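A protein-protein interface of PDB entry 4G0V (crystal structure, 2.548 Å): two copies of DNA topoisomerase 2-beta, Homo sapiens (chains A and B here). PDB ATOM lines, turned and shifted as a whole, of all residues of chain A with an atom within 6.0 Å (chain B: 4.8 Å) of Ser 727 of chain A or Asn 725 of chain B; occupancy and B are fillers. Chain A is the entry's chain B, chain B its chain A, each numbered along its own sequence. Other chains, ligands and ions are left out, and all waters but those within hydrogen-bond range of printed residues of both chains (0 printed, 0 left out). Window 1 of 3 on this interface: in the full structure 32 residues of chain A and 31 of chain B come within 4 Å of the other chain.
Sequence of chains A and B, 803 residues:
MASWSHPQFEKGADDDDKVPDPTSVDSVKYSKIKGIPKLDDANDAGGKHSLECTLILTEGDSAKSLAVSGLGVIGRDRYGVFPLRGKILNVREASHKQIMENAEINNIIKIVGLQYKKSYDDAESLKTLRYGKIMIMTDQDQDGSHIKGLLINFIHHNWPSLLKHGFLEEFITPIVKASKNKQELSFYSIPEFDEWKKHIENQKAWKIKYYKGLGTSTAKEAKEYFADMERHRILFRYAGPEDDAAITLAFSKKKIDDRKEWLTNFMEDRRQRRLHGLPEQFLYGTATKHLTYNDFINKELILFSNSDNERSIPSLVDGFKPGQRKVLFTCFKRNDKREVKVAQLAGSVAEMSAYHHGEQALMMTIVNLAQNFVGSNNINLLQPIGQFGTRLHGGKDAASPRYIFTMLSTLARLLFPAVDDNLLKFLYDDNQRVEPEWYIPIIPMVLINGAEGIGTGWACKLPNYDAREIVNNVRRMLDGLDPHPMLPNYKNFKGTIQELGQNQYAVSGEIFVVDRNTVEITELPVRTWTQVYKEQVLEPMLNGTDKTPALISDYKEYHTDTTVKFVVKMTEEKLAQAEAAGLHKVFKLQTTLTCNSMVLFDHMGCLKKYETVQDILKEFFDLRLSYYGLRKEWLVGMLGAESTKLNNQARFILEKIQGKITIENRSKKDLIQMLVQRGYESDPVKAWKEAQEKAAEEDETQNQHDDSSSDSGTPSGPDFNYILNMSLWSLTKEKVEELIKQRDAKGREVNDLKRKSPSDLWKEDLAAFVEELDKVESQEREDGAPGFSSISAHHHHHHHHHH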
ATOM      1  N   LEU A 724      -5.743   3.623 -21.214  1.00  0.00           N
ATOM      2  CA  LEU A 724      -5.563   3.544 -19.770  1.00  0.00           C
ATOM      3  C   LEU A 724      -4.780   2.322 -19.236  1.00  0.00           C
ATOM      4  O   LEU A 724      -4.294   2.369 -18.111  1.00  0.00           O
ATOM      5  CB  LEU A 724      -6.912   3.708 -19.076  1.00  0.00           C
ATOM      6  CG  LEU A 724      -7.458   5.132 -19.283  1.00  0.00           C
ATOM      7  CD1 LEU A 724      -8.953   5.234 -18.993  1.00  0.00           C
ATOM      8  CD2 LEU A 724      -6.674   6.132 -18.435  1.00  0.00           C
ATOM      9  N   ASN A 725      -4.636   1.255 -20.028  1.00  0.00           N
ATOM     10  CA  ASN A 725      -3.753   0.152 -19.653  1.00  0.00           C
ATOM     11  C   ASN A 725      -2.269   0.434 -19.861  1.00  0.00           C
ATOM     12  O   ASN A 725      -1.440  -0.367 -19.463  1.00  0.00           O
ATOM     13  CB  ASN A 725      -4.085  -1.141 -20.393  1.00  0.00           C
ATOM     14  CG  ASN A 725      -5.395  -1.753 -19.962  1.00  0.00           C
ATOM     15  OD1 ASN A 725      -5.971  -1.376 -18.956  1.00  0.00           O
ATOM     16  ND2 ASN A 725      -5.871  -2.712 -20.732  1.00  0.00           N
ATOM     17  N   MET A 726      -1.919   1.535 -20.507  1.00  0.00           N
ATOM     18  CA  MET A 726      -0.505   1.877 -20.654  1.00  0.00           C
ATOM     19  C   MET A 726       0.149   2.054 -19.279  1.00  0.00           C
ATOM     20  O   MET A 726      -0.504   2.423 -18.304  1.00  0.00           O
ATOM     21  CB  MET A 726      -0.340   3.147 -21.483  1.00  0.00           C
ATOM     22  CG  MET A 726      -0.890   3.045 -22.908  1.00  0.00           C
ATOM     23  SD  MET A 726      -0.682   4.585 -23.832  1.00  0.00           S
ATOM     24  CE  MET A 726       0.980   4.335 -24.437  1.00  0.00           C
ATOM     25  N   SER A 727       1.440   1.781 -19.196  1.00  0.00           N
ATOM     26  CA  SER A 727       2.116   1.825 -17.912  1.00  0.00           C
ATOM     27  C   SER A 727       2.440   3.267 -17.566  1.00  0.00           C
ATOM     28  O   SER A 727       2.545   4.113 -18.449  1.00  0.00           O
ATOM     29  CB  SER A 727       3.414   1.028 -17.965  1.00  0.00           C
ATOM     30  OG  SER A 727       4.375   1.735 -18.728  1.00  0.00           O
ATOM     31  N   LEU A 728       2.624   3.539 -16.276  1.00  0.00           N
ATOM     32  CA  LEU A 728       3.084   4.846 -15.838  1.00  0.00           C
ATOM     33  C   LEU A 728       4.374   5.241 -16.546  1.00  0.00           C
ATOM     34  O   LEU A 728       4.648   6.420 -16.683  1.00  0.00           O
ATOM     35  CB  LEU A 728       3.288   4.866 -14.321  1.00  0.00           C
ATOM     36  CG  LEU A 728       2.007   4.729 -13.490  1.00  0.00           C
ATOM     37  CD1 LEU A 728       2.326   4.539 -12.011  1.00  0.00           C
ATOM     38  CD2 LEU A 728       1.081   5.914 -13.695  1.00  0.00           C
ATOM     39  N   TRP A 729       5.158   4.257 -16.991  1.00  0.00           N
ATOM     40  CA  TRP A 729       6.411   4.526 -17.702  1.00  0.00           C
ATOM     41  C   TRP A 729       6.163   5.385 -18.931  1.00  0.00           C
ATOM     42  O   TRP A 729       7.067   6.076 -19.398  1.00  0.00           O
ATOM     43  CB  TRP A 729       7.069   3.237 -18.180  1.00  0.00           C
ATOM     44  CG  TRP A 729       7.975   2.539 -17.206  1.00  0.00           C
ATOM     45  CD1 TRP A 729       7.850   1.259 -16.758  1.00  0.00           C
ATOM     46  CD2 TRP A 729       9.166   3.060 -16.598  1.00  0.00           C
ATOM     47  NE1 TRP A 729       8.879   0.953 -15.905  1.00  0.00           N
ATOM     48  CE2 TRP A 729       9.699   2.041 -15.786  1.00  0.00           C
ATOM     49  CE3 TRP A 729       9.829   4.289 -16.657  1.00  0.00           C
ATOM     50  CZ2 TRP A 729      10.855   2.212 -15.032  1.00  0.00           C
ATOM     51  CZ3 TRP A 729      10.986   4.456 -15.911  1.00  0.00           C
ATOM     52  CH2 TRP A 729      11.486   3.422 -15.109  1.00  0.00           C
ATOM     53  N   SER A 730       4.936   5.320 -19.450  1.00  0.00           N
ATOM     54  CA  SER A 730       4.554   6.010 -20.678  1.00  0.00           C
ATOM     55  C   SER A 730       4.754   7.510 -20.579  1.00  0.00           C
ATOM     56  O   SER A 730       4.990   8.172 -21.582  1.00  0.00           O
ATOM     57  CB  SER A 730       3.085   5.754 -20.995  1.00  0.00           C
ATOM     58  OG  SER A 730       2.790   4.377 -20.925  1.00  0.00           O
ATOM     59  N   LEU A 731       4.647   8.043 -19.368  1.00  0.00           N
ATOM     60  CA  LEU A 731       4.685   9.483 -19.176  1.00  0.00           C
ATOM     61  C   LEU A 731       6.114   9.989 -19.095  1.00  0.00           C
ATOM     62  O   LEU A 731       6.339  11.189 -18.990  1.00  0.00           O
ATOM     63  CB  LEU A 731       3.915   9.870 -17.920  1.00  0.00           C
ATOM     64  CG  LEU A 731       2.466   9.376 -17.852  1.00  0.00           C
ATOM     65  CD1 LEU A 731       1.800   9.802 -16.549  1.00  0.00           C
ATOM     66  CD2 LEU A 731       1.671   9.889 -19.055  1.00  0.00           C
ATOM     67  N   ASN B 721      10.264  -1.030 -11.199  1.00  0.00           N
ATOM     68  CA  ASN B 721       9.295  -1.452 -12.206  1.00  0.00           C
ATOM     69  C   ASN B 721       7.954  -1.864 -11.636  1.00  0.00           C
ATOM     70  O   ASN B 721       6.936  -1.659 -12.280  1.00  0.00           O
ATOM     71  CB  ASN B 721       9.855  -2.536 -13.134  1.00  0.00           C
ATOM     72  CG  ASN B 721      10.933  -2.001 -14.056  1.00  0.00           C
ATOM     73  OD1 ASN B 721      10.684  -1.105 -14.856  1.00  0.00           O
ATOM     74  ND2 ASN B 721      12.140  -2.530 -13.936  1.00  0.00           N
ATOM     75  N   TYR B 722       7.943  -2.415 -10.422  1.00  0.00           N
ATOM     76  CA  TYR B 722       6.695  -2.843  -9.800  1.00  0.00           C
ATOM     77  C   TYR B 722       5.780  -1.645  -9.554  1.00  0.00           C
ATOM     78  O   TYR B 722       4.567  -1.792  -9.425  1.00  0.00           O
ATOM     79  CB  TYR B 722       6.951  -3.611  -8.493  1.00  0.00           C
ATOM     80  CG  TYR B 722       7.440  -2.768  -7.328  1.00  0.00           C
ATOM     81  CD1 TYR B 722       6.592  -2.446  -6.275  1.00  0.00           C
ATOM     82  CD2 TYR B 722       8.749  -2.309  -7.274  1.00  0.00           C
ATOM     83  CE1 TYR B 722       7.038  -1.686  -5.206  1.00  0.00           C
ATOM     84  CE2 TYR B 722       9.201  -1.550  -6.206  1.00  0.00           C
ATOM     85  CZ  TYR B 722       8.344  -1.244  -5.177  1.00  0.00           C
ATOM     86  OH  TYR B 722       8.794  -0.487  -4.113  1.00  0.00           O
ATOM     87  N   ILE B 723       6.375  -0.459  -9.494  1.00  0.00           N
ATOM     88  CA  ILE B 723       5.605   0.770  -9.404  1.00  0.00           C
ATOM     89  C   ILE B 723       5.256   1.290 -10.807  1.00  0.00           C
ATOM     90  O   ILE B 723       4.086   1.392 -11.186  1.00  0.00           O
ATOM     91  CB  ILE B 723       6.386   1.849  -8.617  1.00  0.00           C
ATOM     92  CG1 ILE B 723       6.760   1.325  -7.229  1.00  0.00           C
ATOM     93  CG2 ILE B 723       5.580   3.122  -8.498  1.00  0.00           C
ATOM     94  CD1 ILE B 723       7.669   2.231  -6.473  1.00  0.00           C
ATOM     95  N   LEU B 724       6.274   1.602 -11.587  1.00  0.00           N
ATOM     96  CA  LEU B 724       6.035   2.282 -12.844  1.00  0.00           C
ATOM     97  C   LEU B 724       5.391   1.413 -13.933  1.00  0.00           C
ATOM     98  O   LEU B 724       4.922   1.945 -14.937  1.00  0.00           O
ATOM     99  CB  LEU B 724       7.316   2.961 -13.318  1.00  0.00           C
ATOM    100  CG  LEU B 724       7.762   4.049 -12.322  1.00  0.00           C
ATOM    101  CD1 LEU B 724       9.219   4.414 -12.504  1.00  0.00           C
ATOM    102  CD2 LEU B 724       6.894   5.291 -12.442  1.00  0.00           C
ATOM    103  N   ASN B 725       5.348   0.094 -13.738  1.00  0.00           N
ATOM    104  CA  ASN B 725       4.602  -0.778 -14.651  1.00  0.00           C
ATOM    105  C   ASN B 725       3.112  -0.780 -14.369  1.00  0.00           C
ATOM    106  O   ASN B 725       2.347  -1.423 -15.077  1.00  0.00           O
ATOM    107  CB  ASN B 725       5.064  -2.237 -14.585  1.00  0.00           C
ATOM    108  CG  ASN B 725       6.419  -2.461 -15.202  1.00  0.00           C
ATOM    109  OD1 ASN B 725       6.976  -1.581 -15.845  1.00  0.00           O
ATOM    110  ND2 ASN B 725       6.952  -3.667 -15.023  1.00  0.00           N
ATOM    111  N   MET B 726       2.694  -0.111 -13.307  1.00  0.00           N
ATOM    112  CA  MET B 726       1.271  -0.045 -13.013  1.00  0.00           C
ATOM    113  C   MET B 726       0.587   0.729 -14.136  1.00  0.00           C
ATOM    114  O   MET B 726       1.187   1.615 -14.744  1.00  0.00           O
ATOM    115  CB  MET B 726       1.023   0.609 -11.652  1.00  0.00           C
ATOM    116  CG  MET B 726       1.371  -0.278 -10.451  1.00  0.00           C
ATOM    117  SD  MET B 726       0.839   0.450  -8.887  1.00  0.00           S
ATOM    118  CE  MET B 726       2.059   1.748  -8.704  1.00  0.00           C
ATOM    119  N   SER B 727      -0.653   0.366 -14.430  1.00  0.00           N
ATOM    120  CA  SER B 727      -1.396   1.014 -15.494  1.00  0.00           C
ATOM    121  C   SER B 727      -1.819   2.411 -15.066  1.00  0.00           C
ATOM    122  O   SER B 727      -1.774   2.749 -13.881  1.00  0.00           O
ATOM    123  CB  SER B 727      -2.632   0.203 -15.852  1.00  0.00           C
ATOM    124  OG  SER B 727      -3.485   0.122 -14.728  1.00  0.00           O
ATOM    125  N   LEU B 728      -2.225   3.217 -16.043  1.00  0.00           N
ATOM    126  CA  LEU B 728      -2.754   4.547 -15.789  1.00  0.00           C
ATOM    127  C   LEU B 728      -4.053   4.452 -14.998  1.00  0.00           C
ATOM    128  O   LEU B 728      -4.373   5.348 -14.234  1.00  0.00           O
ATOM    129  CB  LEU B 728      -2.971   5.294 -17.105  1.00  0.00           C
ATOM    130  CG  LEU B 728      -1.695   5.710 -17.838  1.00  0.00           C
ATOM    131  CD1 LEU B 728      -2.021   6.393 -19.141  1.00  0.00           C
ATOM    132  CD2 LEU B 728      -0.876   6.644 -16.971  1.00  0.00           C
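OD1 of Asn 721 of chain B is in hydrogen-bond range of NE1 of Trp 729 of chain A, at 2.9 Å.
The backbone NH (N) of Trp 729 of chain A lies within hydrogen-bond range of the backbone carbonyl oxygen (O) of Leu 724 of chain B (3.1 Å).
The backbone NH (N) of Leu 728 of chain A sits at hydrogen-bond distance from the backbone carbonyl oxygen (O) of Met 726 of chain B (2.8 Å).
The side-chain amide oxygen of Asn 725 of chain B lies close to the indole nitrogen of Trp 729 of chain A (3.2 Å).
The backbone carbonyl oxygen (O) of Leu 724 of chain A sits at hydrogen-bond distance from the backbone NH (N) of Leu 728 of chain B, 3.0 Å away.
The backbone NH (N) of Leu 728 of chain B sits at hydrogen-bond distance from the backbone carbonyl oxygen (O) of Met 726 of chain A (3.0 Å).
O of Leu 724 of chain B lies within hydrogen-bond range of N of Leu 728 of chain A (3.1 Å).
The side-chain hydroxyl of Ser 730 of chain A sits at hydrogen-bond distance from the backbone carbonyl oxygen of Ser 727 of chain A (2.5 Å).
N of Trp 729 of chain A lies close to OG of Ser 727 of chain A, 3.2 Å away.
The backbone carbonyl oxygen (O) of Asn 721 of chain B sits close to the side-chain amide nitrogen (ND2) of Asn 725 of chain B, at 3.4 Å.
O of Leu 724 of chain A touches CB of Ser 727 of chain B, at 3.5 Å.
O of Asn 725 of chain A touches CB of Ser 727 of chain B, 3.8 Å away.
Ser 727 of chain B touches Met 726 of chain A (CA to O, 3.3 Å).
CB of Ser 727 of chain A touches O of Leu 724 of chain B, 3.5 Å away.
Ser 727 of chain A touches Asn 725 of chain B (CB to O, 3.9 Å).
Met 726 of chain B touches Ser 727 of chain A (O to CA, 3.3 Å).
Leu 728 of chain A touches Ile 723 of chain B.
CD2 of Leu 728 of chain A touches CD2 of Leu 728 of chain B, 3.9 Å away.
Of the printed residues of chain B, Met 726 of chain A touches Ser 727 and Leu 728.
Ser 727 of chain A touches just these residues of chain B: Leu 724 (3.5 Å), Asn 725 (3.9 Å) and Met 726 (3.3 Å).
Of the printed residues of chain A, Asn 721 of chain B touches Trp 729.
Of the printed residues of chain A, Leu 724 of chain B touches Ser 727, Leu 728 and Trp 729.
Asn 725 of chain B touches just these residues of chain A: Ser 727 and Trp 729.
Of the printed residues of chain A, Met 726 of chain B touches Ser 727 (3.3 Å) and Leu 728 (2.8 Å).
Printed residues of chain A within 4 Å of Ser 727 of chain B: Leu 724, Asn 725 and Met 726.
The nearest printed residue of chain B that does not touch Met 726 of chain A is Met 726 of chain B (4.02 Å).
Hydrophobic or aromatic side chains of chain B within 4 Å of the printed part of chain A: Leu 724 and Leu 728.
Printed residues of chain A that touch a printed residue of chain B: Leu 724, Asn 725, Met 726, Ser 727, Leu 728 and Trp 729.
Leu 724 of chain A touches Leu 728 of chain B, and with the chains exchanged Leu 728 of chain A touches Leu 724 of chain B.
Asn 725 of chain A touches Ser 727 of chain B, and with the chains exchanged Ser 727 of chain A touches Asn 725 of chain B.
Met 726 of chain A touches Ser 727 of chain B, and with the chains exchanged Ser 727 of chain A touches Met 726 of chain B.
Leu 728 of chain B touches its own counterpart, Leu 728 of chain A.
5 positions are printed for both chains.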
